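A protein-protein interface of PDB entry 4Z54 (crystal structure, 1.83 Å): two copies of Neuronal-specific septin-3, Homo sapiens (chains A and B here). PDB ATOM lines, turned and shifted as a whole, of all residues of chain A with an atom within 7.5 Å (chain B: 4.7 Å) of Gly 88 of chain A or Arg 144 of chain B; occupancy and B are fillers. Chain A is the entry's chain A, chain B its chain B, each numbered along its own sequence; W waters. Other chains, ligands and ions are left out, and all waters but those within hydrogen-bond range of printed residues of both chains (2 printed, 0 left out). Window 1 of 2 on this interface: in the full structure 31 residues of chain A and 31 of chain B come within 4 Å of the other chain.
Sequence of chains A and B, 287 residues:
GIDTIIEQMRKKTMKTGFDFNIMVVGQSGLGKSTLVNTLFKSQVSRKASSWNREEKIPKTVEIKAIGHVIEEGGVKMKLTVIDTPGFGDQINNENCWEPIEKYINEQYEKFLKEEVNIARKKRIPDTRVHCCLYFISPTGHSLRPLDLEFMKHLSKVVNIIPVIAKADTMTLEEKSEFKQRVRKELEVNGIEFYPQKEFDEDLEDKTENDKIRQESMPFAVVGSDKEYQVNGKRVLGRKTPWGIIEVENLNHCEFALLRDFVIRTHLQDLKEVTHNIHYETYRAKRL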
ATOM      1  N   GLY A  26     -21.111 -29.615 -14.796  1.00  0.00           N
ATOM      2  CA  GLY A  26     -20.574 -28.268 -14.766  1.00  0.00           C
ATOM      3  C   GLY A  26     -19.160 -28.271 -14.232  1.00  0.00           C
ATOM      4  O   GLY A  26     -18.654 -29.313 -13.823  1.00  0.00           O
ATOM      5  N   GLN A  27     -18.515 -27.109 -14.224  1.00  0.00           N
ATOM      6  CA  GLN A  27     -17.154 -27.041 -13.709  1.00  0.00           C
ATOM      7  C   GLN A  27     -17.120 -27.307 -12.209  1.00  0.00           C
ATOM      8  O   GLN A  27     -18.142 -27.202 -11.528  1.00  0.00           O
ATOM      9  CB  GLN A  27     -16.535 -25.686 -14.050  1.00  0.00           C
ATOM     10  CG  GLN A  27     -16.656 -25.411 -15.539  1.00  0.00           C
ATOM     11  CD  GLN A  27     -15.772 -24.285 -16.017  1.00  0.00           C
ATOM     12  OE1 GLN A  27     -14.807 -23.915 -15.352  1.00  0.00           O
ATOM     13  NE2 GLN A  27     -16.102 -23.733 -17.186  1.00  0.00           N
ATOM     14  N   SER A  28     -15.951 -27.689 -11.697  1.00  0.00           N
ATOM     15  CA  SER A  28     -15.844 -28.016 -10.281  1.00  0.00           C
ATOM     16  C   SER A  28     -16.004 -26.763  -9.438  1.00  0.00           C
ATOM     17  O   SER A  28     -15.631 -25.665  -9.863  1.00  0.00           O
ATOM     18  CB  SER A  28     -14.505 -28.690  -9.967  1.00  0.00           C
ATOM     19  OG  SER A  28     -14.518 -30.043 -10.390  1.00  0.00           O
ATOM     20  N   LYS A  59     -13.986 -33.496  -3.554  1.00  0.00           N
ATOM     21  CA  LYS A  59     -14.061 -33.200  -4.972  1.00  0.00           C
ATOM     22  C   LYS A  59     -14.504 -34.460  -5.706  1.00  0.00           C
ATOM     23  O   LYS A  59     -14.052 -35.558  -5.394  1.00  0.00           O
ATOM     24  CB  LYS A  59     -12.698 -32.706  -5.485  1.00  0.00           C
ATOM     25  CG  LYS A  59     -12.691 -32.378  -6.951  1.00  0.00           C
ATOM     26  CD  LYS A  59     -11.346 -31.820  -7.402  1.00  0.00           C
ATOM     27  CE  LYS A  59     -11.377 -31.529  -8.903  1.00  0.00           C
ATOM     28  NZ  LYS A  59     -10.104 -30.931  -9.394  1.00  0.00           N
ATOM     29  N   GLY A  86     -15.815 -32.414 -12.542  1.00  0.00           N
ATOM     30  CA  GLY A  86     -15.763 -31.146 -13.226  1.00  0.00           C
ATOM     31  C   GLY A  86     -14.774 -31.186 -14.372  1.00  0.00           C
ATOM     32  O   GLY A  86     -14.173 -32.218 -14.675  1.00  0.00           O
ATOM     33  N   PHE A  87     -14.627 -30.054 -15.011  1.00  0.00           N
ATOM     34  CA  PHE A  87     -13.833 -29.914 -16.188  1.00  0.00           C
ATOM     35  C   PHE A  87     -13.523 -28.443 -16.374  1.00  0.00           C
ATOM     36  O   PHE A  87     -14.050 -27.620 -15.700  1.00  0.00           O
ATOM     37  CB  PHE A  87     -14.588 -30.431 -17.393  1.00  0.00           C
ATOM     38  CG  PHE A  87     -15.985 -29.963 -17.450  1.00  0.00           C
ATOM     39  CD1 PHE A  87     -16.290 -28.772 -17.984  1.00  0.00           C
ATOM     40  CD2 PHE A  87     -16.985 -30.727 -16.942  1.00  0.00           C
ATOM     41  CE1 PHE A  87     -17.589 -28.335 -18.021  1.00  0.00           C
ATOM     42  CE2 PHE A  87     -18.284 -30.301 -16.977  1.00  0.00           C
ATOM     43  CZ  PHE A  87     -18.584 -29.100 -17.505  1.00  0.00           C
ATOM     44  N   GLY A  88     -12.676 -28.148 -17.328  1.00  0.00           N
ATOM     45  CA  GLY A  88     -12.349 -26.799 -17.682  1.00  0.00           C
ATOM     46  C   GLY A  88     -11.193 -26.205 -16.916  1.00  0.00           C
ATOM     47  O   GLY A  88     -10.872 -25.059 -17.088  1.00  0.00           O
ATOM     48  N   ASP A  89     -10.579 -27.000 -16.080  1.00  0.00           N
ATOM     49  CA  ASP A  89      -9.527 -26.539 -15.212  1.00  0.00           C
ATOM     50  C   ASP A  89      -8.112 -26.754 -15.747  1.00  0.00           C
ATOM     51  O   ASP A  89      -7.147 -26.455 -15.074  1.00  0.00           O
ATOM     52  CB  ASP A  89      -9.670 -27.217 -13.863  1.00  0.00           C
ATOM     53  CG  ASP A  89      -9.750 -28.743 -13.980  1.00  0.00           C
ATOM     54  OD1 ASP A  89     -10.186 -29.279 -15.021  1.00  0.00           O
ATOM     55  OD2 ASP A  89      -9.391 -29.421 -13.010  1.00  0.00           O
ATOM     56  N   GLN A  90      -8.012 -27.330 -16.934  1.00  0.00           N
ATOM     57  CA  GLN A  90      -6.728 -27.628 -17.528  1.00  0.00           C
ATOM     58  C   GLN A  90      -6.307 -26.565 -18.494  1.00  0.00           C
ATOM     59  O   GLN A  90      -7.062 -25.739 -18.849  1.00  0.00           O
ATOM     60  CB  GLN A  90      -6.703 -28.981 -18.248  1.00  0.00           C
ATOM     61  CG  GLN A  90      -7.320 -30.129 -17.513  1.00  0.00           C
ATOM     62  CD  GLN A  90      -6.555 -30.520 -16.303  1.00  0.00           C
ATOM     63  OE1 GLN A  90      -5.361 -30.474 -16.280  1.00  0.00           O
ATOM     64  NE2 GLN A  90      -7.256 -30.915 -15.286  1.00  0.00           N
ATOM     65  N   ILE A  91      -5.063 -26.635 -18.904  1.00  0.00           N
ATOM     66  CA  ILE A  91      -4.546 -25.789 -19.968  1.00  0.00           C
ATOM     67  C   ILE A  91      -5.316 -26.065 -21.248  1.00  0.00           C
ATOM     68  O   ILE A  91      -5.689 -25.151 -21.979  1.00  0.00           O
ATOM     69  CB  ILE A  91      -3.064 -26.039 -20.206  1.00  0.00           C
ATOM     70  CG1 ILE A  91      -2.266 -25.683 -18.945  1.00  0.00           C
ATOM     71  CG2 ILE A  91      -2.577 -25.224 -21.398  1.00  0.00           C
ATOM     72  CD1 ILE A  91      -0.793 -26.028 -19.023  1.00  0.00           C
ATOM     73  N   ASN A  92      -5.567 -27.343 -21.494  1.00  0.00           N
ATOM     74  CA  ASN A  92      -6.238 -27.783 -22.708  1.00  0.00           C
ATOM     75  C   ASN A  92      -7.484 -28.573 -22.370  1.00  0.00           C
ATOM     76  O   ASN A  92      -7.394 -29.701 -21.890  1.00  0.00           O
ATOM     77  CB  ASN A  92      -5.276 -28.619 -23.556  1.00  0.00           C
ATOM     78  CG  ASN A  92      -5.945 -29.233 -24.770  1.00  0.00           C
ATOM     79  OD1 ASN A  92      -7.018 -28.811 -25.179  1.00  0.00           O
ATOM     80  ND2 ASN A  92      -5.303 -30.234 -25.355  1.00  0.00           N
ATOM     81  N   ASN A  93      -8.652 -27.991 -22.624  1.00  0.00           N
ATOM     82  CA  ASN A  93      -9.905 -28.661 -22.280  1.00  0.00           C
ATOM     83  C   ASN A  93     -10.710 -29.154 -23.483  1.00  0.00           C
ATOM     84  O   ASN A  93     -11.908 -29.435 -23.354  1.00  0.00           O
ATOM     85  CB  ASN A  93     -10.771 -27.734 -21.448  1.00  0.00           C
ATOM     86  CG  ASN A  93     -10.008 -27.138 -20.296  1.00  0.00           C
ATOM     87  OD1 ASN A  93      -9.714 -27.828 -19.320  1.00  0.00           O
ATOM     88  ND2 ASN A  93      -9.649 -25.856 -20.411  1.00  0.00           N
ATOM     89  N   CYS A  96     -13.489 -32.181 -23.462  1.00  0.00           N
ATOM     90  CA  CYS A  96     -13.717 -32.565 -22.076  1.00  0.00           C
ATOM     91  C   CYS A  96     -15.151 -33.031 -21.843  1.00  0.00           C
ATOM     92  O   CYS A  96     -15.482 -33.506 -20.755  1.00  0.00           O
ATOM     93  CB  CYS A  96     -13.383 -31.409 -21.121  1.00  0.00           C
ATOM     94  SG  CYS A  96     -14.392 -29.929 -21.363  1.00  0.00           S
ATOM     95  N   ARG A 144     -19.263 -18.494 -20.175  1.00  0.00           N
ATOM     96  CA  ARG A 144     -17.927 -18.933 -20.540  1.00  0.00           C
ATOM     97  C   ARG A 144     -18.021 -19.748 -21.827  1.00  0.00           C
ATOM     98  O   ARG A 144     -18.951 -20.554 -21.997  1.00  0.00           O
ATOM     99  CB  ARG A 144     -17.295 -19.750 -19.413  1.00  0.00           C
ATOM    100  CG  ARG A 144     -17.201 -19.009 -18.073  1.00  0.00           C
ATOM    101  CD  ARG A 144     -16.057 -19.572 -17.226  1.00  0.00           C
ATOM    102  NE  ARG A 144     -15.925 -18.946 -15.900  1.00  0.00           N
ATOM    103  CZ  ARG A 144     -15.409 -17.735 -15.681  1.00  0.00           C
ATOM    104  NH1 ARG A 144     -15.018 -16.985 -16.694  1.00  0.00           N
ATOM    105  NH2 ARG A 144     -15.314 -17.256 -14.443  1.00  0.00           N
ATOM    106  N   LEU A 146     -16.396 -22.298 -22.878  1.00  0.00           N
ATOM    107  CA  LEU A 146     -16.410 -23.740 -22.657  1.00  0.00           C
ATOM    108  C   LEU A 146     -17.813 -24.218 -22.279  1.00  0.00           C
ATOM    109  O   LEU A 146     -18.250 -25.285 -22.719  1.00  0.00           O
ATOM    110  CB  LEU A 146     -15.405 -24.146 -21.577  1.00  0.00           C
ATOM    111  CG  LEU A 146     -15.319 -25.643 -21.264  1.00  0.00           C
ATOM    112  CD1 LEU A 146     -15.249 -26.482 -22.541  1.00  0.00           C
ATOM    113  CD2 LEU A 146     -14.080 -25.882 -20.449  1.00  0.00           C
ATOM    114  N   PHE A 150     -19.944 -26.939 -24.390  1.00  0.00           N
ATOM    115  CA  PHE A 150     -20.352 -28.127 -23.647  1.00  0.00           C
ATOM    116  C   PHE A 150     -21.875 -28.325 -23.723  1.00  0.00           C
ATOM    117  O   PHE A 150     -22.361 -29.424 -24.018  1.00  0.00           O
ATOM    118  CB  PHE A 150     -19.880 -28.003 -22.192  1.00  0.00           C
ATOM    119  CG  PHE A 150     -19.583 -29.320 -21.523  1.00  0.00           C
ATOM    120  CD1 PHE A 150     -20.585 -30.249 -21.311  1.00  0.00           C
ATOM    121  CD2 PHE A 150     -18.293 -29.617 -21.083  1.00  0.00           C
ATOM    122  CE1 PHE A 150     -20.315 -31.465 -20.690  1.00  0.00           C
ATOM    123  CE2 PHE A 150     -18.027 -30.826 -20.458  1.00  0.00           C
ATOM    124  CZ  PHE A 150     -19.057 -31.755 -20.261  1.00  0.00           C
ATOM    125  N   GLN B  27      -9.341 -14.996 -14.269  1.00  0.00           N
ATOM    126  CA  GLN B  27     -10.458 -15.260 -15.165  1.00  0.00           C
ATOM    127  C   GLN B  27     -11.408 -14.086 -15.137  1.00  0.00           C
ATOM    128  O   GLN B  27     -11.483 -13.348 -14.144  1.00  0.00           O
ATOM    129  CB  GLN B  27     -11.239 -16.518 -14.769  1.00  0.00           C
ATOM    130  CG  GLN B  27     -10.457 -17.789 -14.550  1.00  0.00           C
ATOM    131  CD  GLN B  27     -11.409 -18.912 -14.184  1.00  0.00           C
ATOM    132  OE1 GLN B  27     -12.231 -19.323 -15.000  1.00  0.00           O
ATOM    133  NE2 GLN B  27     -11.330 -19.383 -12.943  1.00  0.00           N
ATOM    134  N   GLY B  88      -7.173 -17.332 -19.084  1.00  0.00           N
ATOM    135  CA  GLY B  88      -7.220 -18.619 -18.418  1.00  0.00           C
ATOM    136  C   GLY B  88      -8.658 -19.049 -18.150  1.00  0.00           C
ATOM    137  O   GLY B  88      -8.937 -19.744 -17.180  1.00  0.00           O
ATOM    138  N   SER B 142      -9.089 -28.242  -4.720  1.00  0.00           N
ATOM    139  CA  SER B 142      -7.695 -28.030  -5.108  1.00  0.00           C
ATOM    140  C   SER B 142      -7.603 -27.005  -6.241  1.00  0.00           C
ATOM    141  O   SER B 142      -8.504 -26.930  -7.080  1.00  0.00           O
ATOM    142  CB  SER B 142      -7.048 -29.354  -5.528  1.00  0.00           C
ATOM    143  OG  SER B 142      -7.835 -30.027  -6.495  1.00  0.00           O
ATOM    144  N   LEU B 143      -6.524 -26.217  -6.247  1.00  0.00           N
ATOM    145  CA  LEU B 143      -6.321 -25.160  -7.244  1.00  0.00           C
ATOM    146  C   LEU B 143      -6.337 -25.744  -8.666  1.00  0.00           C
ATOM    147  O   LEU B 143      -5.870 -26.860  -8.882  1.00  0.00           O
ATOM    148  CB  LEU B 143      -4.994 -24.420  -6.988  1.00  0.00           C
ATOM    149  CG  LEU B 143      -4.805 -23.556  -5.724  1.00  0.00           C
ATOM    150  CD1 LEU B 143      -3.334 -23.243  -5.499  1.00  0.00           C
ATOM    151  CD2 LEU B 143      -5.572 -22.263  -5.833  1.00  0.00           C
ATOM    152  N   ARG B 144      -6.876 -24.995  -9.629  1.00  0.00           N
ATOM    153  CA  ARG B 144      -6.824 -25.423 -11.031  1.00  0.00           C
ATOM    154  C   ARG B 144      -5.386 -25.526 -11.512  1.00  0.00           C
ATOM    155  O   ARG B 144      -4.597 -24.601 -11.289  1.00  0.00           O
ATOM    156  CB  ARG B 144      -7.576 -24.447 -11.935  1.00  0.00           C
ATOM    157  CG  ARG B 144      -9.007 -24.095 -11.496  1.00  0.00           C
ATOM    158  CD  ARG B 144      -9.695 -23.283 -12.600  1.00  0.00           C
ATOM    159  NE  ARG B 144      -8.904 -22.102 -12.945  1.00  0.00           N
ATOM    160  CZ  ARG B 144      -8.941 -21.489 -14.124  1.00  0.00           C
ATOM    161  NH1 ARG B 144      -9.735 -21.944 -15.094  1.00  0.00           N
ATOM    162  NH2 ARG B 144      -8.174 -20.422 -14.333  1.00  0.00           N
ATOM    163  N   PRO B 145      -5.037 -26.639 -12.176  1.00  0.00           N
ATOM    164  CA  PRO B 145      -3.744 -26.736 -12.863  1.00  0.00           C
ATOM    165  C   PRO B 145      -3.436 -25.505 -13.724  1.00  0.00           C
ATOM    166  O   PRO B 145      -2.290 -25.040 -13.765  1.00  0.00           O
ATOM    167  CB  PRO B 145      -3.914 -27.987 -13.732  1.00  0.00           C
ATOM    168  CG  PRO B 145      -4.810 -28.856 -12.908  1.00  0.00           C
ATOM    169  CD  PRO B 145      -5.777 -27.919 -12.214  1.00  0.00           C
ATOM    170  N   LEU B 146      -4.457 -24.966 -14.381  1.00  0.00           N
ATOM    171  CA  LEU B 146      -4.267 -23.772 -15.194  1.00  0.00           C
ATOM    172  C   LEU B 146      -3.811 -22.579 -14.355  1.00  0.00           C
ATOM    173  O   LEU B 146      -2.913 -21.850 -14.766  1.00  0.00           O
ATOM    174  CB  LEU B 146      -5.545 -23.425 -15.941  1.00  0.00           C
ATOM    175  CG  LEU B 146      -5.514 -22.239 -16.899  1.00  0.00           C
ATOM    176  CD1 LEU B 146      -4.357 -22.329 -17.886  1.00  0.00           C
ATOM    177  CD2 LEU B 146      -6.834 -22.158 -17.630  1.00  0.00           C
ATOM    178  N   ASP B 147      -4.427 -22.371 -13.196  1.00  0.00           N
ATOM    179  CA  ASP B 147      -3.995 -21.281 -12.309  1.00  0.00           C
ATOM    180  C   ASP B 147      -2.574 -21.483 -11.809  1.00  0.00           C
ATOM    181  O   ASP B 147      -1.795 -20.527 -11.703  1.00  0.00           O
ATOM    182  CB  ASP B 147      -4.920 -21.141 -11.108  1.00  0.00           C
ATOM    183  CG  ASP B 147      -6.243 -20.508 -11.469  1.00  0.00           C
ATOM    184  OD1 ASP B 147      -6.255 -19.602 -12.334  1.00  0.00           O
ATOM    185  OD2 ASP B 147      -7.261 -20.924 -10.888  1.00  0.00           O
ATOM    186  N   LEU B 148      -2.238 -22.721 -11.473  1.00  0.00           N
ATOM    187  CA  LEU B 148      -0.875 -23.018 -11.045  1.00  0.00           C
ATOM    188  C   LEU B 148       0.122 -22.693 -12.152  1.00  0.00           C
ATOM    189  O   LEU B 148       1.176 -22.119 -11.901  1.00  0.00           O
ATOM    190  CB  LEU B 148      -0.736 -24.473 -10.645  1.00  0.00           C
ATOM    191  CG  LEU B 148      -1.509 -24.883  -9.399  1.00  0.00           C
ATOM    192  CD1 LEU B 148      -1.493 -26.398  -9.289  1.00  0.00           C
ATOM    193  CD2 LEU B 148      -0.883 -24.227  -8.189  1.00  0.00           C
HETATM  194  O   HOH W   1     -11.930 -23.440 -15.047  1.00  0.00           O
HETATM  195  O   HOH W   2     -13.812 -21.248 -15.850  1.00  0.00           O
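The backbone carbonyl oxygen of Asp 89 of chain A is in hydrogen-bond range of the backbone NH of Leu 146 of chain B (3.2 Å).
The backbone carbonyl oxygen (O) of Gly 88 of chain B is in hydrogen-bond range of the guanidinium group (NH2) of Arg 144 of chain B, at 3.0 Å.
The backbone NH of Asp 89 of chain A sits at hydrogen-bond distance from the side-chain amide oxygen of Asn 93 of chain A (3.5 Å).
The side-chain amino group (NZ) of Lys 59 of chain A is in salt-bridge range of the side-chain carboxylate (OD2) of Asp 89 of chain A (3.98 Å).
OD2 of Asp 147 of chain B is in salt-bridge range of NE of Arg 144 of chain B (2.9 Å).
The backbone NH of Gln 90 of chain A sits at hydrogen-bond distance from the side-chain amide oxygen of Asn 93 of chain A, 3.0 Å away.
NE2 of Gln 90 of chain A lies within hydrogen-bond range of OD1 of Asp 89 of chain A.
OG of Ser 142 of chain B touches NZ of Lys 59 of chain A (3.8 Å).
Arg 144 of chain B touches Gly 88 of chain A (NH1 to O, 3.9 Å).
Asp 89 of chain A touches Arg 144 of chain B (O to CB, 3.8 Å).
Pro 145 of chain B touches Asp 89 of chain A.
Gln 90 of chain A touches Pro 145 of chain B (OE1 to CG, 3.8 Å).
Leu 146 of chain B touches Gln 90 of chain A (CD2 to O, 3.8 Å).
Arg 144 of chain A touches Gln 27 of chain B.
Gly 88 of chain A touches just one residue of chain B: Arg 144.
Of the printed residues of chain B, Gln 90 of chain A touches Pro 145 (3.8 Å) and Leu 146 (3.8 Å).
Cys 96 of chain A touches none of the printed residues of chain B.
Printed residues of chain B within 4 Å of Arg 144 of chain A: Gln 27.
Printed residues of chain A within 4 Å of Gln 27 of chain B: Arg 144 (3.6 Å).
Of the printed residues of chain A, Pro 145 of chain B touches Asp 89 (3.5 Å) and Gln 90 (3.8 Å).
Of the printed residues of chain A, Leu 146 of chain B touches Asp 89 and Gln 90.
Leu 148 of chain B touches none of the printed residues of chain A.
The nearest residue of chain A that does not touch Arg 144 of chain B is Gln 27 of chain A (5.4 Å).
The nearest printed residue of chain B that does not touch Asp 89 of chain A is Asp 147 of chain B (5.3 Å).
Hydrophobic or aromatic side chains of chain B within 4 Å of the printed part of chain A: Pro 145 and Leu 146.
Of the 16 printed residues of chain A, 5 touch a printed residue of chain B.
Among the printed residues, 8 pairs touch across the chains.
Among the printed residues, no Asp or Glu carboxylate lies within 4 Å of a Lys or Arg side-chain nitrogen of the other chain.
Gly 88 of chain A touches Arg 144 of chain B, but with the chains exchanged Arg 144 of chain A does not touch Gly 88 of chain B (6.7 Å).
Arg 144 of chain A touches Gln 27 of chain B, but with the chains exchanged Gln 27 of chain A does not touch Arg 144 of chain B (5.4 Å).
4 positions are printed for both chains.
Of the 8 pairs that touch across the chains among the printed residues, none has its exchanged pair printed and touching as well.
Water W2 lies within hydrogen-bond range of the side-chain amide oxygen of Gln 27 of chain B (2.6 Å), the side-chain amide oxygen of Gln 27 of chain A (2.9 Å) and the guanidinium group of Arg 144 of chain A (3.1 Å).
Water W1 lies within hydrogen-bond range of the guanidinium group (NH1) of Arg 144 of chain B (2.7 Å), the backbone carbonyl oxygen (O) of Gly 88 of chain A (2.8 Å) and the side-chain amide oxygen (OE1) of Gln 27 of chain A (2.9 Å).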
